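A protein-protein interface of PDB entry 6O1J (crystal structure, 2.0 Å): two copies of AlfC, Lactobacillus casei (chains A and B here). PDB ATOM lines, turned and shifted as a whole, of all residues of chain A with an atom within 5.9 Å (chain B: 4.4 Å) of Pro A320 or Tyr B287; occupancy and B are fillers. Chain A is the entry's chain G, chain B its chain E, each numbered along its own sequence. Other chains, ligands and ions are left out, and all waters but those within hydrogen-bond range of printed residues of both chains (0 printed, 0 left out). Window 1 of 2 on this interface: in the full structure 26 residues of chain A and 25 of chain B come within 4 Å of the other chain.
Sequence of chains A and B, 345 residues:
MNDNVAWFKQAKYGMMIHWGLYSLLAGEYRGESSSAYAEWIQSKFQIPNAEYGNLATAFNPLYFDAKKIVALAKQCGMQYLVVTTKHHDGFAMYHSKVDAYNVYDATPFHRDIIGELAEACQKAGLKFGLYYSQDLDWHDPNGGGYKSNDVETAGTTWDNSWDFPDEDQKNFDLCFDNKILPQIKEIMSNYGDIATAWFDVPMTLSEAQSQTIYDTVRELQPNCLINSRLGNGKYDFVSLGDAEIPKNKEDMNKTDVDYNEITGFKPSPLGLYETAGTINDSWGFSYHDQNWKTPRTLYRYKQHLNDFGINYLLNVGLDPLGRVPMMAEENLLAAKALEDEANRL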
ATOM      1  N   TRP A  19     -26.850 -24.689  12.986  1.00  0.00           N
ATOM      2  CA  TRP A  19     -25.447 -24.983  13.344  1.00  0.00           C
ATOM      3  C   TRP A  19     -25.066 -26.369  12.843  1.00  0.00           C
ATOM      4  O   TRP A  19     -25.798 -27.317  13.141  1.00  0.00           O
ATOM      5  CB  TRP A  19     -25.266 -24.866  14.854  1.00  0.00           C
ATOM      6  CG  TRP A  19     -23.854 -24.582  15.238  1.00  0.00           C
ATOM      7  CD1 TRP A  19     -22.904 -23.926  14.512  1.00  0.00           C
ATOM      8  CD2 TRP A  19     -23.242 -24.931  16.482  1.00  0.00           C
ATOM      9  NE1 TRP A  19     -21.737 -23.842  15.223  1.00  0.00           N
ATOM     10  CE2 TRP A  19     -21.917 -24.455  16.431  1.00  0.00           C
ATOM     11  CE3 TRP A  19     -23.687 -25.602  17.631  1.00  0.00           C
ATOM     12  CZ2 TRP A  19     -21.033 -24.638  17.484  1.00  0.00           C
ATOM     13  CZ3 TRP A  19     -22.802 -25.786  18.672  1.00  0.00           C
ATOM     14  CH2 TRP A  19     -21.503 -25.293  18.598  1.00  0.00           C
ATOM     15  N   SER A  23     -21.245 -24.582   8.891  1.00  0.00           N
ATOM     16  CA  SER A  23     -20.866 -23.355   9.630  1.00  0.00           C
ATOM     17  C   SER A  23     -19.361 -23.090   9.549  1.00  0.00           C
ATOM     18  O   SER A  23     -18.977 -21.881   9.586  1.00  0.00           O
ATOM     19  CB  SER A  23     -21.337 -23.397  11.066  1.00  0.00           C
ATOM     20  OG  SER A  23     -22.694 -23.828  11.124  1.00  0.00           O
ATOM     21  N   LEU A  24     -18.548 -24.137   9.402  1.00  0.00           N
ATOM     22  CA  LEU A  24     -17.058 -23.990   9.358  1.00  0.00           C
ATOM     23  C   LEU A  24     -16.626 -23.398   8.011  1.00  0.00           C
ATOM     24  O   LEU A  24     -15.714 -22.586   8.033  1.00  0.00           O
ATOM     25  CB  LEU A  24     -16.382 -25.334   9.626  1.00  0.00           C
ATOM     26  CG  LEU A  24     -16.665 -26.017  10.969  1.00  0.00           C
ATOM     27  CD1 LEU A  24     -15.603 -27.097  11.240  1.00  0.00           C
ATOM     28  CD2 LEU A  24     -16.676 -25.037  12.128  1.00  0.00           C
ATOM     29  N   ALA A  26     -18.472 -21.423   6.220  1.00  0.00           N
ATOM     30  CA  ALA A  26     -18.929 -20.045   6.459  1.00  0.00           C
ATOM     31  C   ALA A  26     -19.213 -19.334   5.136  1.00  0.00           C
ATOM     32  O   ALA A  26     -18.861 -18.157   5.016  1.00  0.00           O
ATOM     33  CB  ALA A  26     -17.897 -19.321   7.290  1.00  0.00           C
ATOM     34  N   PHE A  59     -14.231 -29.458  14.027  1.00  0.00           N
ATOM     35  CA  PHE A  59     -15.377 -28.864  14.762  1.00  0.00           C
ATOM     36  C   PHE A  59     -15.039 -28.848  16.250  1.00  0.00           C
ATOM     37  O   PHE A  59     -15.160 -29.899  16.907  1.00  0.00           O
ATOM     38  CB  PHE A  59     -16.671 -29.619  14.450  1.00  0.00           C
ATOM     39  CG  PHE A  59     -17.923 -28.925  14.934  1.00  0.00           C
ATOM     40  CD1 PHE A  59     -18.378 -29.127  16.230  1.00  0.00           C
ATOM     41  CD2 PHE A  59     -18.627 -28.070  14.112  1.00  0.00           C
ATOM     42  CE1 PHE A  59     -19.521 -28.482  16.681  1.00  0.00           C
ATOM     43  CE2 PHE A  59     -19.772 -27.428  14.566  1.00  0.00           C
ATOM     44  CZ  PHE A  59     -20.213 -27.634  15.844  1.00  0.00           C
ATOM     45  N   ASN A  60     -14.592 -27.702  16.762  1.00  0.00           N
ATOM     46  CA  ASN A  60     -14.198 -27.518  18.183  1.00  0.00           C
ATOM     47  C   ASN A  60     -14.603 -26.115  18.626  1.00  0.00           C
ATOM     48  O   ASN A  60     -13.755 -25.249  18.854  1.00  0.00           O
ATOM     49  CB  ASN A  60     -12.701 -27.831  18.386  1.00  0.00           C
ATOM     50  CG  ASN A  60     -12.396 -28.194  19.820  1.00  0.00           C
ATOM     51  OD1 ASN A  60     -13.315 -28.385  20.597  1.00  0.00           O
ATOM     52  ND2 ASN A  60     -11.126 -28.333  20.178  1.00  0.00           N
ATOM     53  N   PRO A  61     -15.924 -25.840  18.729  1.00  0.00           N
ATOM     54  CA  PRO A  61     -16.426 -24.517  19.099  1.00  0.00           C
ATOM     55  C   PRO A  61     -16.236 -24.162  20.583  1.00  0.00           C
ATOM     56  O   PRO A  61     -17.159 -24.318  21.364  1.00  0.00           O
ATOM     57  CB  PRO A  61     -17.908 -24.626  18.727  1.00  0.00           C
ATOM     58  CG  PRO A  61     -18.232 -26.083  18.942  1.00  0.00           C
ATOM     59  CD  PRO A  61     -17.007 -26.789  18.421  1.00  0.00           C
ATOM     60  N   LEU A  62     -15.053 -23.638  20.924  1.00  0.00           N
ATOM     61  CA  LEU A  62     -14.619 -23.411  22.326  1.00  0.00           C
ATOM     62  C   LEU A  62     -15.539 -22.428  23.043  1.00  0.00           C
ATOM     63  O   LEU A  62     -15.545 -22.481  24.273  1.00  0.00           O
ATOM     64  CB  LEU A  62     -13.176 -22.907  22.350  1.00  0.00           C
ATOM     65  CG  LEU A  62     -12.153 -23.829  21.681  1.00  0.00           C
ATOM     66  CD1 LEU A  62     -10.771 -23.209  21.732  1.00  0.00           C
ATOM     67  CD2 LEU A  62     -12.171 -25.230  22.303  1.00  0.00           C
ATOM     68  N   PHE A 285     -24.360 -19.780   9.194  1.00  0.00           N
ATOM     69  CA  PHE A 285     -23.321 -18.728   9.275  1.00  0.00           C
ATOM     70  C   PHE A 285     -22.626 -18.576   7.919  1.00  0.00           C
ATOM     71  O   PHE A 285     -22.193 -19.553   7.255  1.00  0.00           O
ATOM     72  CB  PHE A 285     -22.331 -19.042  10.389  1.00  0.00           C
ATOM     73  CG  PHE A 285     -21.247 -18.008  10.524  1.00  0.00           C
ATOM     74  CD1 PHE A 285     -21.529 -16.765  11.056  1.00  0.00           C
ATOM     75  CD2 PHE A 285     -19.970 -18.246  10.038  1.00  0.00           C
ATOM     76  CE1 PHE A 285     -20.543 -15.798  11.159  1.00  0.00           C
ATOM     77  CE2 PHE A 285     -18.983 -17.271  10.153  1.00  0.00           C
ATOM     78  CZ  PHE A 285     -19.262 -16.054  10.725  1.00  0.00           C
ATOM     79  N   TYR A 287     -19.663 -15.773   6.408  1.00  0.00           N
ATOM     80  CA  TYR A 287     -18.902 -14.576   6.846  1.00  0.00           C
ATOM     81  C   TYR A 287     -19.124 -13.461   5.808  1.00  0.00           C
ATOM     82  O   TYR A 287     -19.186 -12.343   6.313  1.00  0.00           O
ATOM     83  CB  TYR A 287     -17.521 -14.967   7.346  1.00  0.00           C
ATOM     84  CG  TYR A 287     -16.481 -14.815   6.295  1.00  0.00           C
ATOM     85  CD1 TYR A 287     -16.020 -13.549   5.968  1.00  0.00           C
ATOM     86  CD2 TYR A 287     -15.841 -15.907   5.726  1.00  0.00           C
ATOM     87  CE1 TYR A 287     -15.017 -13.364   5.023  1.00  0.00           C
ATOM     88  CE2 TYR A 287     -14.852 -15.746   4.762  1.00  0.00           C
ATOM     89  CZ  TYR A 287     -14.410 -14.471   4.442  1.00  0.00           C
ATOM     90  OH  TYR A 287     -13.458 -14.304   3.497  1.00  0.00           O
ATOM     91  N   GLN A 290     -23.077  -9.796   5.388  1.00  0.00           N
ATOM     92  CA  GLN A 290     -23.233  -8.742   6.437  1.00  0.00           C
ATOM     93  C   GLN A 290     -24.522  -7.964   6.210  1.00  0.00           C
ATOM     94  O   GLN A 290     -24.590  -6.825   6.698  1.00  0.00           O
ATOM     95  CB  GLN A 290     -22.023  -7.803   6.403  1.00  0.00           C
ATOM     96  CG  GLN A 290     -20.720  -8.534   6.590  1.00  0.00           C
ATOM     97  CD  GLN A 290     -20.636  -9.190   7.942  1.00  0.00           C
ATOM     98  OE1 GLN A 290     -21.097  -8.648   8.916  1.00  0.00           O
ATOM     99  NE2 GLN A 290     -20.048 -10.373   8.024  1.00  0.00           N
ATOM    100  N   LEU A 318     -24.984 -19.825  14.213  1.00  0.00           N
ATOM    101  CA  LEU A 318     -23.791 -19.793  15.080  1.00  0.00           C
ATOM    102  C   LEU A 318     -22.524 -19.941  14.228  1.00  0.00           C
ATOM    103  O   LEU A 318     -22.503 -20.690  13.229  1.00  0.00           O
ATOM    104  CB  LEU A 318     -23.875 -20.883  16.149  1.00  0.00           C
ATOM    105  CG  LEU A 318     -25.056 -20.781  17.110  1.00  0.00           C
ATOM    106  CD1 LEU A 318     -25.095 -21.975  18.039  1.00  0.00           C
ATOM    107  CD2 LEU A 318     -25.029 -19.483  17.902  1.00  0.00           C
ATOM    108  N   ASP A 319     -21.475 -19.261  14.642  1.00  0.00           N
ATOM    109  CA  ASP A 319     -20.198 -19.186  13.910  1.00  0.00           C
ATOM    110  C   ASP A 319     -19.397 -20.447  14.242  1.00  0.00           C
ATOM    111  O   ASP A 319     -19.882 -21.321  14.967  1.00  0.00           O
ATOM    112  CB  ASP A 319     -19.548 -17.827  14.166  1.00  0.00           C
ATOM    113  CG  ASP A 319     -18.718 -17.718  15.419  1.00  0.00           C
ATOM    114  OD1 ASP A 319     -18.639 -18.686  16.181  1.00  0.00           O
ATOM    115  OD2 ASP A 319     -18.214 -16.610  15.630  1.00  0.00           O
ATOM    116  N   PRO A 320     -18.203 -20.629  13.659  1.00  0.00           N
ATOM    117  CA  PRO A 320     -17.387 -21.821  13.923  1.00  0.00           C
ATOM    118  C   PRO A 320     -16.981 -22.025  15.392  1.00  0.00           C
ATOM    119  O   PRO A 320     -16.675 -23.154  15.736  1.00  0.00           O
ATOM    120  CB  PRO A 320     -16.112 -21.592  13.090  1.00  0.00           C
ATOM    121  CG  PRO A 320     -16.565 -20.675  11.986  1.00  0.00           C
ATOM    122  CD  PRO A 320     -17.589 -19.752  12.648  1.00  0.00           C
ATOM    123  N   LEU A 321     -16.943 -20.956  16.203  1.00  0.00           N
ATOM    124  CA  LEU A 321     -16.559 -21.060  17.628  1.00  0.00           C
ATOM    125  C   LEU A 321     -17.798 -21.237  18.502  1.00  0.00           C
ATOM    126  O   LEU A 321     -17.635 -21.255  19.729  1.00  0.00           O
ATOM    127  CB  LEU A 321     -15.728 -19.833  18.020  1.00  0.00           C
ATOM    128  CG  LEU A 321     -14.295 -19.848  17.502  1.00  0.00           C
ATOM    129  CD1 LEU A 321     -13.581 -18.561  17.905  1.00  0.00           C
ATOM    130  CD2 LEU A 321     -13.540 -21.058  18.057  1.00  0.00           C
ATOM    131  N   GLY A 322     -18.980 -21.386  17.886  1.00  0.00           N
ATOM    132  CA  GLY A 322     -20.252 -21.624  18.599  1.00  0.00           C
ATOM    133  C   GLY A 322     -20.905 -20.330  19.048  1.00  0.00           C
ATOM    134  O   GLY A 322     -21.720 -20.385  19.994  1.00  0.00           O
ATOM    135  N   ARG A 323     -20.590 -19.211  18.381  1.00  0.00           N
ATOM    136  CA  ARG A 323     -20.966 -17.863  18.868  1.00  0.00           C
ATOM    137  C   ARG A 323     -22.139 -17.329  18.039  1.00  0.00           C
ATOM    138  O   ARG A 323     -22.209 -17.592  16.810  1.00  0.00           O
ATOM    139  CB  ARG A 323     -19.798 -16.875  18.788  1.00  0.00           C
ATOM    140  CG  ARG A 323     -18.588 -17.251  19.616  1.00  0.00           C
ATOM    141  CD  ARG A 323     -17.387 -16.312  19.460  1.00  0.00           C
ATOM    142  NE  ARG A 323     -16.917 -16.175  18.082  1.00  0.00           N
ATOM    143  CZ  ARG A 323     -15.928 -15.376  17.708  1.00  0.00           C
ATOM    144  NH1 ARG A 323     -15.379 -14.567  18.578  1.00  0.00           N
ATOM    145  NH2 ARG A 323     -15.527 -15.315  16.452  1.00  0.00           N
ATOM    146  N   ALA B  26     -11.396 -13.979  14.818  1.00  0.00           N
ATOM    147  CA  ALA B  26     -11.836 -13.344  13.563  1.00  0.00           C
ATOM    148  C   ALA B  26     -12.472 -11.982  13.860  1.00  0.00           C
ATOM    149  O   ALA B  26     -13.500 -11.680  13.247  1.00  0.00           O
ATOM    150  CB  ALA B  26     -12.778 -14.283  12.825  1.00  0.00           C
ATOM    151  N   GLU B  28     -13.695 -10.647  16.717  1.00  0.00           N
ATOM    152  CA  GLU B  28     -14.878 -10.679  17.601  1.00  0.00           C
ATOM    153  C   GLU B  28     -14.526 -11.404  18.897  1.00  0.00           C
ATOM    154  O   GLU B  28     -13.882 -12.481  18.809  1.00  0.00           O
ATOM    155  CB  GLU B  28     -15.967 -11.434  16.848  1.00  0.00           C
ATOM    156  CG  GLU B  28     -17.350 -11.026  17.205  1.00  0.00           C
ATOM    157  CD  GLU B  28     -18.284 -11.532  16.125  1.00  0.00           C
ATOM    158  OE1 GLU B  28     -17.947 -11.414  14.936  1.00  0.00           O
ATOM    159  OE2 GLU B  28     -19.273 -12.121  16.488  1.00  0.00           O
ATOM    160  N   PHE B 285      -7.174 -11.859  10.008  1.00  0.00           N
ATOM    161  CA  PHE B 285      -8.536 -12.140   9.516  1.00  0.00           C
ATOM    162  C   PHE B 285      -9.581 -11.555  10.464  1.00  0.00           C
ATOM    163  O   PHE B 285      -9.518 -11.747  11.716  1.00  0.00           O
ATOM    164  CB  PHE B 285      -8.719 -13.638   9.308  1.00  0.00           C
ATOM    165  CG  PHE B 285     -10.086 -14.008   8.806  1.00  0.00           C
ATOM    166  CD1 PHE B 285     -10.445 -13.733   7.506  1.00  0.00           C
ATOM    167  CD2 PHE B 285     -11.049 -14.535   9.663  1.00  0.00           C
ATOM    168  CE1 PHE B 285     -11.713 -14.038   7.032  1.00  0.00           C
ATOM    169  CE2 PHE B 285     -12.317 -14.836   9.199  1.00  0.00           C
ATOM    170  CZ  PHE B 285     -12.656 -14.573   7.881  1.00  0.00           C
ATOM    171  N   SER B 286     -10.587 -10.877   9.887  1.00  0.00           N
ATOM    172  CA  SER B 286     -11.708 -10.315  10.666  1.00  0.00           C
ATOM    173  C   SER B 286     -13.014 -10.502   9.900  1.00  0.00           C
ATOM    174  O   SER B 286     -13.093  -9.884   8.822  1.00  0.00           O
ATOM    175  CB  SER B 286     -11.490  -8.856  10.946  1.00  0.00           C
ATOM    176  OG  SER B 286     -12.624  -8.303  11.620  1.00  0.00           O
ATOM    177  N   TYR B 287     -13.972 -11.266  10.442  1.00  0.00           N
ATOM    178  CA  TYR B 287     -15.289 -11.559   9.801  1.00  0.00           C
ATOM    179  C   TYR B 287     -15.971 -10.235   9.423  1.00  0.00           C
ATOM    180  O   TYR B 287     -16.462 -10.091   8.281  1.00  0.00           O
ATOM    181  CB  TYR B 287     -16.303 -12.268  10.725  1.00  0.00           C
ATOM    182  CG  TYR B 287     -16.040 -13.709  11.078  1.00  0.00           C
ATOM    183  CD1 TYR B 287     -15.506 -14.589  10.145  1.00  0.00           C
ATOM    184  CD2 TYR B 287     -16.304 -14.199  12.353  1.00  0.00           C
ATOM    185  CE1 TYR B 287     -15.241 -15.901  10.468  1.00  0.00           C
ATOM    186  CE2 TYR B 287     -16.040 -15.523  12.690  1.00  0.00           C
ATOM    187  CZ  TYR B 287     -15.507 -16.378  11.740  1.00  0.00           C
ATOM    188  OH  TYR B 287     -15.182 -17.694  11.987  1.00  0.00           O
ATOM    189  N   HIS B 288     -15.959  -9.279  10.350  1.00  0.00           N
ATOM    190  CA  HIS B 288     -16.803  -8.044  10.260  1.00  0.00           C
ATOM    191  C   HIS B 288     -16.175  -7.015   9.314  1.00  0.00           C
ATOM    192  O   HIS B 288     -16.916  -6.130   8.849  1.00  0.00           O
ATOM    193  CB  HIS B 288     -17.123  -7.473  11.644  1.00  0.00           C
ATOM    194  CG  HIS B 288     -15.980  -6.869  12.396  1.00  0.00           C
ATOM    195  ND1 HIS B 288     -15.622  -5.533  12.268  1.00  0.00           N
ATOM    196  CD2 HIS B 288     -15.164  -7.395  13.337  1.00  0.00           C
ATOM    197  CE1 HIS B 288     -14.612  -5.267  13.063  1.00  0.00           C
ATOM    198  NE2 HIS B 288     -14.316  -6.400  13.737  1.00  0.00           N
ATOM    199  N   ASP B 289     -14.889  -7.137   8.997  1.00  0.00           N
ATOM    200  CA  ASP B 289     -14.187  -6.151   8.134  1.00  0.00           C
ATOM    201  C   ASP B 289     -14.315  -6.597   6.671  1.00  0.00           C
ATOM    202  O   ASP B 289     -13.500  -7.408   6.201  1.00  0.00           O
ATOM    203  CB  ASP B 289     -12.741  -5.929   8.581  1.00  0.00           C
ATOM    204  CG  ASP B 289     -12.031  -4.902   7.713  1.00  0.00           C
ATOM    205  OD1 ASP B 289     -12.659  -4.404   6.737  1.00  0.00           O
ATOM    206  OD2 ASP B 289     -10.862  -4.629   7.961  1.00  0.00           O
ATOM    207  N   GLN B 290     -15.278  -6.015   5.972  1.00  0.00           N
ATOM    208  CA  GLN B 290     -15.496  -6.223   4.526  1.00  0.00           C
ATOM    209  C   GLN B 290     -15.057  -4.986   3.752  1.00  0.00           C
ATOM    210  O   GLN B 290     -15.551  -4.831   2.645  1.00  0.00           O
ATOM    211  CB  GLN B 290     -16.979  -6.521   4.273  1.00  0.00           C
ATOM    212  CG  GLN B 290     -17.459  -7.736   5.044  1.00  0.00           C
ATOM    213  CD  GLN B 290     -16.753  -8.979   4.590  1.00  0.00           C
ATOM    214  OE1 GLN B 290     -16.491  -9.138   3.379  1.00  0.00           O
ATOM    215  NE2 GLN B 290     -16.476  -9.868   5.543  1.00  0.00           N
ATOM    216  N   PRO B 320      -9.712 -19.025   9.537  1.00  0.00           N
ATOM    217  CA  PRO B 320      -9.514 -20.165  10.420  1.00  0.00           C
ATOM    218  C   PRO B 320      -9.240 -21.505   9.723  1.00  0.00           C
ATOM    219  O   PRO B 320      -8.683 -22.394  10.372  1.00  0.00           O
ATOM    220  CB  PRO B 320     -10.822 -20.269  11.212  1.00  0.00           C
ATOM    221  CG  PRO B 320     -11.420 -18.861  11.121  1.00  0.00           C
ATOM    222  CD  PRO B 320     -11.024 -18.371   9.744  1.00  0.00           C
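The backbone carbonyl oxygen (O) of Glu B28 is in hydrogen-bond range of the guanidinium group (NH1) of Arg A323 (2.6 Å).
O of Ala B26 sits at hydrogen-bond distance from N of Tyr B287, at 2.9 Å. The backbone carbonyl oxygen (O) of Tyr B287 sits at hydrogen-bond distance from the side-chain amide nitrogen (NE2) of Gln B290 (2.7 Å). The indole nitrogen (NE1) of Trp A19 sits at hydrogen-bond distance from the backbone carbonyl oxygen (O) of Asp A319 (3.1 Å). The backbone carbonyl oxygen (O) of Ala A26 is in hydrogen-bond range of the backbone NH (N) of Tyr A287 (2.9 Å). OD1 of Asp A319 lies within hydrogen-bond range of N of Leu A321 (2.8 Å). The side-chain carboxylate (OD1) of Asp A319 is in hydrogen-bond range of the backbone NH (N) of Gly A322, 3.2 Å away.
Among the printed residues, pairs that only touch across the chains: Pro A320 with Tyr B287 (3.2 Å), Tyr A287 with Tyr B287 (3.5 Å), Gln A290 with Tyr B287 (3.6 Å), Gln A290 with Gln B290 (3.7 Å), Tyr A287 with Gln B290 (3.7 Å), Tyr A287 with Phe B285 (3.8 Å), Arg A323 with Tyr B287 (3.8 Å), Phe A285 with Tyr B287 (3.8 Å) and Asp A319 with Tyr B287 (3.8 Å).
Pro A320 touches just one residue of chain B: Tyr B287 (3.2 Å). Tyr B287 touches six residues of chain A. Of the printed residues of chain A, Gln B290 touches Tyr A287 and Gln A290. Printed residues of chain B within 4 Å of Tyr A287: Phe B285, Tyr B287 and Gln B290. Of the printed residues of chain A, Phe B285 touches Tyr A287 (3.8 Å).
Of the 17 printed residues of chain A, 6 touch a printed residue of chain B. Printed residues of chain A that touch a printed residue of chain B: Phe A285, Tyr A287, Gln A290, Asp A319, Pro A320 and Arg A323. Printed residues of chain B that touch a printed residue of chain A: Glu B28, Phe B285, Tyr B287 and Gln B290. Among the printed residues, 10 pairs touch across the chains. Among the printed residues, no Asp or Glu carboxylate lies within 4 Å of a Lys or Arg side-chain nitrogen of the other chain.
Phe A285 touches Tyr B287, and with the chains exchanged Tyr A287 touches Phe B285. Tyr B287 touches its own counterpart, Tyr A287. Tyr A287 touches Gln B290, and with the chains exchanged Gln A290 touches Tyr B287. Pro A320 touches Tyr B287, but with the chains exchanged Tyr A287 does not touch Pro B320 (6.7 Å). Of the 10 pairs that touch across the chains among the printed residues, 6 have their exchanged pair printed and touching as well.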
